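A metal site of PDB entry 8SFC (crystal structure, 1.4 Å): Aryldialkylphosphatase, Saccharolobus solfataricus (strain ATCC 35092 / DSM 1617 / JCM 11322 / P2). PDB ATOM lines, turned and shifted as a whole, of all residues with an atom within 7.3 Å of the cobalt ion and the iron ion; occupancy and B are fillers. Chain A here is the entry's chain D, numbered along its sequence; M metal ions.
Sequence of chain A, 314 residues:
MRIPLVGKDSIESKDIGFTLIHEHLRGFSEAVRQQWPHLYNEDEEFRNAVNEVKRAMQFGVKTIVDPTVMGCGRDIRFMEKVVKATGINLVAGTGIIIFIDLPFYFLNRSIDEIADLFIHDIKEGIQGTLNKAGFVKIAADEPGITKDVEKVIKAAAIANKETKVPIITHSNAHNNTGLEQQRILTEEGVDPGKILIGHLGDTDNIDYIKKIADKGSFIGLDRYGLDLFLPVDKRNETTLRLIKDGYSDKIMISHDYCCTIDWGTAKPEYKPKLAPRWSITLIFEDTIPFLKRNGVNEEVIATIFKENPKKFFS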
ATOM      1  N   HIS A  22      13.218  -9.832  23.812  1.00  0.00           N
ATOM      2  CA  HIS A  22      14.597  -9.423  23.543  1.00  0.00           C
ATOM      3  C   HIS A  22      15.032  -9.992  22.200  1.00  0.00           C
ATOM      4  O   HIS A  22      15.649 -11.050  22.164  1.00  0.00           O
ATOM      5  CB  HIS A  22      15.491  -9.928  24.678  1.00  0.00           C
ATOM      6  CG  HIS A  22      16.876  -9.353  24.675  1.00  0.00           C
ATOM      7  ND1 HIS A  22      17.389  -8.650  25.744  1.00  0.00           N
ATOM      8  CD2 HIS A  22      17.852  -9.365  23.733  1.00  0.00           C
ATOM      9  CE1 HIS A  22      18.625  -8.259  25.456  1.00  0.00           C
ATOM     10  NE2 HIS A  22      18.929  -8.687  24.245  1.00  0.00           N
ATOM     11  N   GLU A  23      14.674  -9.323  21.102  1.00  0.00           N
ATOM     12  CA  GLU A  23      15.031  -9.764  19.753  1.00  0.00           C
ATOM     13  C   GLU A  23      15.465  -8.565  18.934  1.00  0.00           C
ATOM     14  O   GLU A  23      14.704  -7.599  18.787  1.00  0.00           O
ATOM     15  CB  GLU A  23      13.833 -10.401  19.044  1.00  0.00           C
ATOM     16  CG  GLU A  23      13.058 -11.415  19.881  1.00  0.00           C
ATOM     17  CD  GLU A  23      13.829 -12.700  20.122  1.00  0.00           C
ATOM     18  OE1 GLU A  23      14.819 -12.969  19.430  1.00  0.00           O
ATOM     19  OE2 GLU A  23      13.410 -13.462  21.025  1.00  0.00           O
ATOM     20  N   HIS A  24      16.635  -8.655  18.316  1.00  0.00           N
ATOM     21  CA  HIS A  24      17.196  -7.554  17.532  1.00  0.00           C
ATOM     22  C   HIS A  24      16.900  -7.744  16.057  1.00  0.00           C
ATOM     23  O   HIS A  24      17.242  -8.783  15.481  1.00  0.00           O
ATOM     24  CB  HIS A  24      18.711  -7.489  17.728  1.00  0.00           C
ATOM     25  CG  HIS A  24      19.136  -7.352  19.150  1.00  0.00           C
ATOM     26  ND1 HIS A  24      19.415  -6.134  19.730  1.00  0.00           N
ATOM     27  CD2 HIS A  24      19.382  -8.293  20.095  1.00  0.00           C
ATOM     28  CE1 HIS A  24      19.774  -6.329  20.993  1.00  0.00           C
ATOM     29  NE2 HIS A  24      19.768  -7.626  21.232  1.00  0.00           N
ATOM     30  N   PRO A  67      15.871  -4.517  21.703  1.00  0.00           N
ATOM     31  CA  PRO A  67      16.682  -3.680  22.606  1.00  0.00           C
ATOM     32  C   PRO A  67      17.965  -3.163  21.977  1.00  0.00           C
ATOM     33  O   PRO A  67      18.972  -2.982  22.687  1.00  0.00           O
ATOM     34  CB  PRO A  67      16.983  -4.628  23.771  1.00  0.00           C
ATOM     35  CG  PRO A  67      17.122  -5.964  23.102  1.00  0.00           C
ATOM     36  CD  PRO A  67      16.139  -5.959  21.912  1.00  0.00           C
ATOM     37  N   THR A  68      17.949  -2.944  20.665  1.00  0.00           N
ATOM     38  CA  THR A  68      19.089  -2.362  19.975  1.00  0.00           C
ATOM     39  C   THR A  68      19.161  -0.870  20.327  1.00  0.00           C
ATOM     40  O   THR A  68      18.192  -0.129  20.120  1.00  0.00           O
ATOM     41  CB  THR A  68      18.909  -2.517  18.467  1.00  0.00           C
ATOM     42  OG1 THR A  68      18.595  -3.885  18.126  1.00  0.00           O
ATOM     43  CG2 THR A  68      20.167  -2.113  17.704  1.00  0.00           C
ATOM     44  N   CYS A  72      24.975  -0.619  19.182  1.00  0.00           N
ATOM     45  CA  CYS A  72      24.509  -1.721  18.369  1.00  0.00           C
ATOM     46  C   CYS A  72      23.739  -1.266  17.159  1.00  0.00           C
ATOM     47  O   CYS A  72      23.176  -2.095  16.444  1.00  0.00           O
ATOM     48  CB  CYS A  72      23.650  -2.680  19.201  1.00  0.00           C
ATOM     49  SG  CYS A  72      24.549  -3.925  20.197  1.00  0.00           S
ATOM     50  N   ILE A  97      25.102   0.573  25.184  1.00  0.00           N
ATOM     51  CA  ILE A  97      25.806  -0.681  25.462  1.00  0.00           C
ATOM     52  C   ILE A  97      27.300  -0.406  25.366  1.00  0.00           C
ATOM     53  O   ILE A  97      27.840  -0.143  24.290  1.00  0.00           O
ATOM     54  CB  ILE A  97      25.385  -1.800  24.488  1.00  0.00           C
ATOM     55  CG1 ILE A  97      23.932  -2.203  24.763  1.00  0.00           C
ATOM     56  CG2 ILE A  97      26.295  -3.008  24.631  1.00  0.00           C
ATOM     57  CD1 ILE A  97      23.301  -2.982  23.644  1.00  0.00           C
ATOM     58  N   PHE A  99      31.128  -1.858  27.361  1.00  0.00           N
ATOM     59  CA  PHE A  99      31.749  -2.780  28.296  1.00  0.00           C
ATOM     60  C   PHE A  99      32.873  -2.151  29.111  1.00  0.00           C
ATOM     61  O   PHE A  99      33.199  -2.675  30.189  1.00  0.00           O
ATOM     62  CB  PHE A  99      32.315  -4.016  27.573  1.00  0.00           C
ATOM     63  CG  PHE A  99      31.273  -4.918  26.937  1.00  0.00           C
ATOM     64  CD1 PHE A  99      29.913  -4.707  27.128  1.00  0.00           C
ATOM     65  CD2 PHE A  99      31.680  -5.974  26.146  1.00  0.00           C
ATOM     66  CE1 PHE A  99      28.976  -5.547  26.532  1.00  0.00           C
ATOM     67  CE2 PHE A  99      30.754  -6.807  25.545  1.00  0.00           C
ATOM     68  CZ  PHE A  99      29.403  -6.590  25.745  1.00  0.00           C
ATOM     69  N   KCX A 137      17.973   0.207  27.897  1.00  0.00           N
ATOM     70  CA  KCX A 137      18.872  -0.942  27.808  1.00  0.00           C
ATOM     71  CB  KCX A 137      18.817  -1.526  26.390  1.00  0.00           C
ATOM     72  CG  KCX A 137      19.875  -2.555  26.074  1.00  0.00           C
ATOM     73  CD  KCX A 137      19.601  -3.868  26.801  1.00  0.00           C
ATOM     74  CE  KCX A 137      20.687  -4.893  26.531  1.00  0.00           C
ATOM     75  NZ  KCX A 137      20.733  -5.288  25.107  1.00  0.00           N
ATOM     76  C   KCX A 137      20.291  -0.528  28.174  1.00  0.00           C
ATOM     77  O   KCX A 137      20.799   0.480  27.668  1.00  0.00           O
ATOM     78  CX  KCX A 137      21.367  -6.372  24.663  1.00  0.00           C
ATOM     79  OQ1 KCX A 137      21.351  -6.610  23.445  1.00  0.00           O
ATOM     80  OQ2 KCX A 137      21.986  -7.128  25.419  1.00  0.00           O
ATOM     81  N   ILE A 138      20.932  -1.299  29.053  1.00  0.00           N
ATOM     82  CA  ILE A 138      22.291  -1.029  29.534  1.00  0.00           C
ATOM     83  C   ILE A 138      23.051  -2.347  29.571  1.00  0.00           C
ATOM     84  O   ILE A 138      22.445  -3.411  29.423  1.00  0.00           O
ATOM     85  CB  ILE A 138      22.277  -0.372  30.929  1.00  0.00           C
ATOM     86  CG1 ILE A 138      21.671  -1.326  31.957  1.00  0.00           C
ATOM     87  CG2 ILE A 138      21.519   0.968  30.888  1.00  0.00           C
ATOM     88  CD1 ILE A 138      21.627  -0.765  33.347  1.00  0.00           C
ATOM     89  N   ALA A 139      24.362  -2.286  29.813  1.00  0.00           N
ATOM     90  CA  ALA A 139      25.182  -3.494  29.744  1.00  0.00           C
ATOM     91  C   ALA A 139      26.342  -3.443  30.732  1.00  0.00           C
ATOM     92  O   ALA A 139      26.764  -2.386  31.215  1.00  0.00           O
ATOM     93  CB  ALA A 139      25.787  -3.668  28.350  1.00  0.00           C
ATOM     94  N   ASP A 141      29.952  -6.440  31.124  1.00  0.00           N
ATOM     95  CA  ASP A 141      30.374  -7.766  30.682  1.00  0.00           C
ATOM     96  C   ASP A 141      31.624  -8.186  31.452  1.00  0.00           C
ATOM     97  O   ASP A 141      31.723  -7.915  32.662  1.00  0.00           O
ATOM     98  CB  ASP A 141      30.621  -7.773  29.167  1.00  0.00           C
ATOM     99  CG  ASP A 141      30.545  -9.175  28.566  1.00  0.00           C
ATOM    100  OD1 ASP A 141      29.419  -9.660  28.279  1.00  0.00           O
ATOM    101  OD2 ASP A 141      31.613  -9.791  28.366  1.00  0.00           O
ATOM    102  N   ILE A 168      16.166  -3.114  30.811  1.00  0.00           N
ATOM    103  CA  ILE A 168      16.684  -4.392  30.372  1.00  0.00           C
ATOM    104  C   ILE A 168      18.197  -4.306  30.418  1.00  0.00           C
ATOM    105  O   ILE A 168      18.768  -3.293  30.014  1.00  0.00           O
ATOM    106  CB  ILE A 168      16.201  -4.698  28.934  1.00  0.00           C
ATOM    107  CG1 ILE A 168      14.674  -4.724  28.884  1.00  0.00           C
ATOM    108  CG2 ILE A 168      16.857  -5.967  28.433  1.00  0.00           C
ATOM    109  CD1 ILE A 168      14.077  -4.925  27.471  1.00  0.00           C
ATOM    110  N   THR A 169      18.864  -5.366  30.889  1.00  0.00           N
ATOM    111  CA  THR A 169      20.314  -5.369  30.891  1.00  0.00           C
ATOM    112  C   THR A 169      20.895  -6.511  30.078  1.00  0.00           C
ATOM    113  O   THR A 169      20.280  -7.567  29.901  1.00  0.00           O
ATOM    114  CB  THR A 169      20.909  -5.438  32.308  1.00  0.00           C
ATOM    115  OG1 THR A 169      20.998  -6.807  32.724  1.00  0.00           O
ATOM    116  CG2 THR A 169      20.060  -4.666  33.270  1.00  0.00           C
ATOM    117  N   HIS A 170      22.099  -6.262  29.580  1.00  0.00           N
ATOM    118  CA  HIS A 170      23.029  -7.290  29.148  1.00  0.00           C
ATOM    119  C   HIS A 170      23.980  -7.517  30.308  1.00  0.00           C
ATOM    120  O   HIS A 170      24.515  -6.559  30.874  1.00  0.00           O
ATOM    121  CB  HIS A 170      23.809  -6.779  27.944  1.00  0.00           C
ATOM    122  CG  HIS A 170      25.025  -7.573  27.597  1.00  0.00           C
ATOM    123  ND1 HIS A 170      25.185  -8.192  26.373  1.00  0.00           N
ATOM    124  CD2 HIS A 170      26.194  -7.775  28.269  1.00  0.00           C
ATOM    125  CE1 HIS A 170      26.357  -8.784  26.331  1.00  0.00           C
ATOM    126  NE2 HIS A 170      26.991  -8.548  27.466  1.00  0.00           N
ATOM    127  N   SER A 171      24.183  -8.782  30.668  1.00  0.00           N
ATOM    128  CA  SER A 171      25.187  -9.117  31.674  1.00  0.00           C
ATOM    129  C   SER A 171      26.017 -10.293  31.188  1.00  0.00           C
ATOM    130  O   SER A 171      25.686 -10.946  30.188  1.00  0.00           O
ATOM    131  CB  SER A 171      24.564  -9.410  33.052  1.00  0.00           C
ATOM    132  OG  SER A 171      24.054 -10.725  33.122  1.00  0.00           O
ATOM    133  N   GLY A 198      19.640  -9.776  31.884  1.00  0.00           N
ATOM    134  CA  GLY A 198      19.709 -10.593  30.709  1.00  0.00           C
ATOM    135  C   GLY A 198      20.949 -11.464  30.615  1.00  0.00           C
ATOM    136  O   GLY A 198      21.938 -11.253  31.311  1.00  0.00           O
ATOM    137  N   HIS A 199      20.851 -12.463  29.740  1.00  0.00           N
ATOM    138  CA  HIS A 199      21.963 -13.318  29.339  1.00  0.00           C
ATOM    139  C   HIS A 199      22.324 -14.350  30.397  1.00  0.00           C
ATOM    140  O   HIS A 199      23.412 -14.921  30.362  1.00  0.00           O
ATOM    141  CB  HIS A 199      23.165 -12.491  28.893  1.00  0.00           C
ATOM    142  CG  HIS A 199      22.899 -11.719  27.651  1.00  0.00           C
ATOM    143  ND1 HIS A 199      21.679 -11.750  27.009  1.00  0.00           N
ATOM    144  CD2 HIS A 199      23.663 -10.838  26.951  1.00  0.00           C
ATOM    145  CE1 HIS A 199      21.712 -10.957  25.947  1.00  0.00           C
ATOM    146  NE2 HIS A 199      22.904 -10.398  25.898  1.00  0.00           N
ATOM    147  N   ASP A 222      17.647 -15.835  27.855  1.00  0.00           N
ATOM    148  CA  ASP A 222      17.424 -15.193  26.564  1.00  0.00           C
ATOM    149  C   ASP A 222      18.633 -15.343  25.651  1.00  0.00           C
ATOM    150  O   ASP A 222      19.007 -14.406  24.938  1.00  0.00           O
ATOM    151  CB  ASP A 222      17.040 -13.728  26.758  1.00  0.00           C
ATOM    152  CG  ASP A 222      18.042 -12.958  27.606  1.00  0.00           C
ATOM    153  OD1 ASP A 222      19.162 -13.476  27.808  1.00  0.00           O
ATOM    154  OD2 ASP A 222      17.710 -11.871  28.115  1.00  0.00           O
ATOM    155  N   ARG A 223      19.262 -16.518  25.649  1.00  0.00           N
ATOM    156  CA  ARG A 223      20.364 -16.800  24.734  1.00  0.00           C
ATOM    157  C   ARG A 223      20.059 -18.011  23.858  1.00  0.00           C
ATOM    158  O   ARG A 223      20.961 -18.530  23.190  1.00  0.00           O
ATOM    159  CB  ARG A 223      21.681 -16.976  25.505  1.00  0.00           C
ATOM    160  CG  ARG A 223      22.948 -17.117  24.672  1.00  0.00           C
ATOM    161  CD  ARG A 223      23.442 -15.780  24.174  1.00  0.00           C
ATOM    162  NE  ARG A 223      24.065 -15.012  25.241  1.00  0.00           N
ATOM    163  CZ  ARG A 223      24.610 -13.819  25.093  1.00  0.00           C
ATOM    164  NH1 ARG A 223      24.567 -13.177  23.930  1.00  0.00           N
ATOM    165  NH2 ARG A 223      25.219 -13.246  26.126  1.00  0.00           N
ATOM    166  N   HIS A 255      15.773 -15.413  22.148  1.00  0.00           N
ATOM    167  CA  HIS A 255      16.927 -15.946  21.416  1.00  0.00           C
ATOM    168  C   HIS A 255      17.940 -14.846  21.165  1.00  0.00           C
ATOM    169  O   HIS A 255      19.125 -15.006  21.487  1.00  0.00           O
ATOM    170  CB  HIS A 255      16.537 -16.378  20.000  1.00  0.00           C
ATOM    171  CG  HIS A 255      15.155 -16.915  19.871  1.00  0.00           C
ATOM    172  ND1 HIS A 255      14.044 -16.148  20.114  1.00  0.00           N
ATOM    173  CD2 HIS A 255      14.701 -18.119  19.442  1.00  0.00           C
ATOM    174  CE1 HIS A 255      12.957 -16.870  19.868  1.00  0.00           C
ATOM    175  NE2 HIS A 255      13.333 -18.061  19.440  1.00  0.00           N
ATOM    176  N   ASP A 256      17.494 -13.770  20.509  1.00  0.00           N
ATOM    177  CA  ASP A 256      18.250 -12.602  20.098  1.00  0.00           C
ATOM    178  C   ASP A 256      19.627 -12.907  19.520  1.00  0.00           C
ATOM    179  O   ASP A 256      19.952 -12.461  18.420  1.00  0.00           O
ATOM    180  CB  ASP A 256      18.315 -11.572  21.236  1.00  0.00           C
ATOM    181  CG  ASP A 256      19.460 -11.793  22.197  1.00  0.00           C
ATOM    182  OD1 ASP A 256      19.356 -12.693  23.054  1.00  0.00           O
ATOM    183  OD2 ASP A 256      20.433 -11.011  22.170  1.00  0.00           O
ATOM    184  N   TYR A 257      20.421 -13.694  20.238  1.00  0.00           N
ATOM    185  CA  TYR A 257      21.881 -13.642  20.204  1.00  0.00           C
ATOM    186  C   TYR A 257      22.328 -12.184  20.297  1.00  0.00           C
ATOM    187  O   TYR A 257      21.708 -11.279  19.725  1.00  0.00           O
ATOM    188  CB  TYR A 257      22.503 -14.415  19.029  1.00  0.00           C
ATOM    189  CG  TYR A 257      22.574 -13.696  17.694  1.00  0.00           C
ATOM    190  CD1 TYR A 257      23.445 -12.634  17.494  1.00  0.00           C
ATOM    191  CD2 TYR A 257      21.773 -14.105  16.638  1.00  0.00           C
ATOM    192  CE1 TYR A 257      23.517 -11.986  16.275  1.00  0.00           C
ATOM    193  CE2 TYR A 257      21.834 -13.464  15.423  1.00  0.00           C
ATOM    194  CZ  TYR A 257      22.703 -12.403  15.238  1.00  0.00           C
ATOM    195  OH  TYR A 257      22.761 -11.771  14.022  1.00  0.00           O
ATOM    196  N   CYS A 258      23.409 -11.948  21.027  1.00  0.00           N
ATOM    197  CA  CYS A 258      23.745 -10.587  21.427  1.00  0.00           C
ATOM    198  C   CYS A 258      23.918  -9.666  20.223  1.00  0.00           C
ATOM    199  O   CYS A 258      24.530 -10.047  19.211  1.00  0.00           O
ATOM    200  CB  CYS A 258      25.023 -10.622  22.236  1.00  0.00           C
ATOM    201  SG  CYS A 258      25.432  -9.051  22.871  1.00  0.00           S
ATOM    202  N   CYS A 259      23.384  -8.443  20.320  1.00  0.00           N
ATOM    203  CA  CYS A 259      23.482  -7.496  19.209  1.00  0.00           C
ATOM    204  C   CYS A 259      24.915  -7.046  18.957  1.00  0.00           C
ATOM    205  O   CYS A 259      25.204  -6.533  17.873  1.00  0.00           O
ATOM    206  CB  CYS A 259      22.628  -6.250  19.412  1.00  0.00           C
ATOM    207  SG  CYS A 259      23.083  -5.217  20.841  1.00  0.00           S
ATOM    208  N   THR A 260      25.804  -7.193  19.945  1.00  0.00           N
ATOM    209  CA  THR A 260      27.201  -6.835  19.759  1.00  0.00           C
ATOM    210  C   THR A 260      27.914  -7.744  18.761  1.00  0.00           C
ATOM    211  O   THR A 260      29.017  -7.410  18.323  1.00  0.00           O
ATOM    212  CB  THR A 260      27.943  -6.821  21.101  1.00  0.00           C
ATOM    213  OG1 THR A 260      28.071  -8.151  21.596  1.00  0.00           O
ATOM    214  CG2 THR A 260      27.172  -5.979  22.114  1.00  0.00           C
HETATM  215 CO    CO M   1      23.864  -8.681  24.932  1.00  0.00          CO
HETATM  216 FE    FE M   2      20.677  -8.375  22.846  1.00  0.00          FE
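The cobalt ion is bound by ND1 of His 170 (2.0 Å), NE2 of His 199 (2.2 Å), OQ2 of KCX 137 (2.5 Å) and SG of Cys 258 (2.6 Å).
The iron ion is bound by OQ1 of KCX 137 (2.0 Å), NE2 of His 24 (2.0 Å) and NE2 of His 22 (2.3 Å). Slightly farther from the iron ion lies the side-chain carboxylate (OD2) of Asp 256 (2.7 Å).
The side-chain hydroxyl (OG1) of Thr 68 lies within hydrogen-bond range of a ring nitrogen (ND1) of His 24, 2.9 Å away. OD1 of Asp 141 lies within hydrogen-bond range of NE2 of His 170 (2.8 Å). The backbone NH of His 199 sits at hydrogen-bond distance from the side-chain carboxylate of Asp 222. OD2 of Asp 256 lies close to NE2 of His 22 (3.5 Å). OD2 of Asp 256 sits at hydrogen-bond distance from N of Cys 258 (3.3 Å). SG of Cys 258 lies close to OG1 of Thr 260, 3.1 Å away. N of Asp 256 sits at hydrogen-bond distance from OE1 of Glu 23 (3.0 Å). The side-chain carboxylate (OD1) of Asp 256 sits close to the backbone carbonyl oxygen (O) of Asp 222 (2.6 Å).
Four residues have an atom within 4 Å of the cobalt ion: KCX 137, His 170, His 199 and Cys 258.
Residues that only touch the iron ion: Cys 259 (3.7 Å). Within 4 Å of the iron ion: His 22, His 24, KCX 137, Asp 256 and Cys 259. The nearest printed residue that does not touch the iron ion is Cys 258 (4.04 Å).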
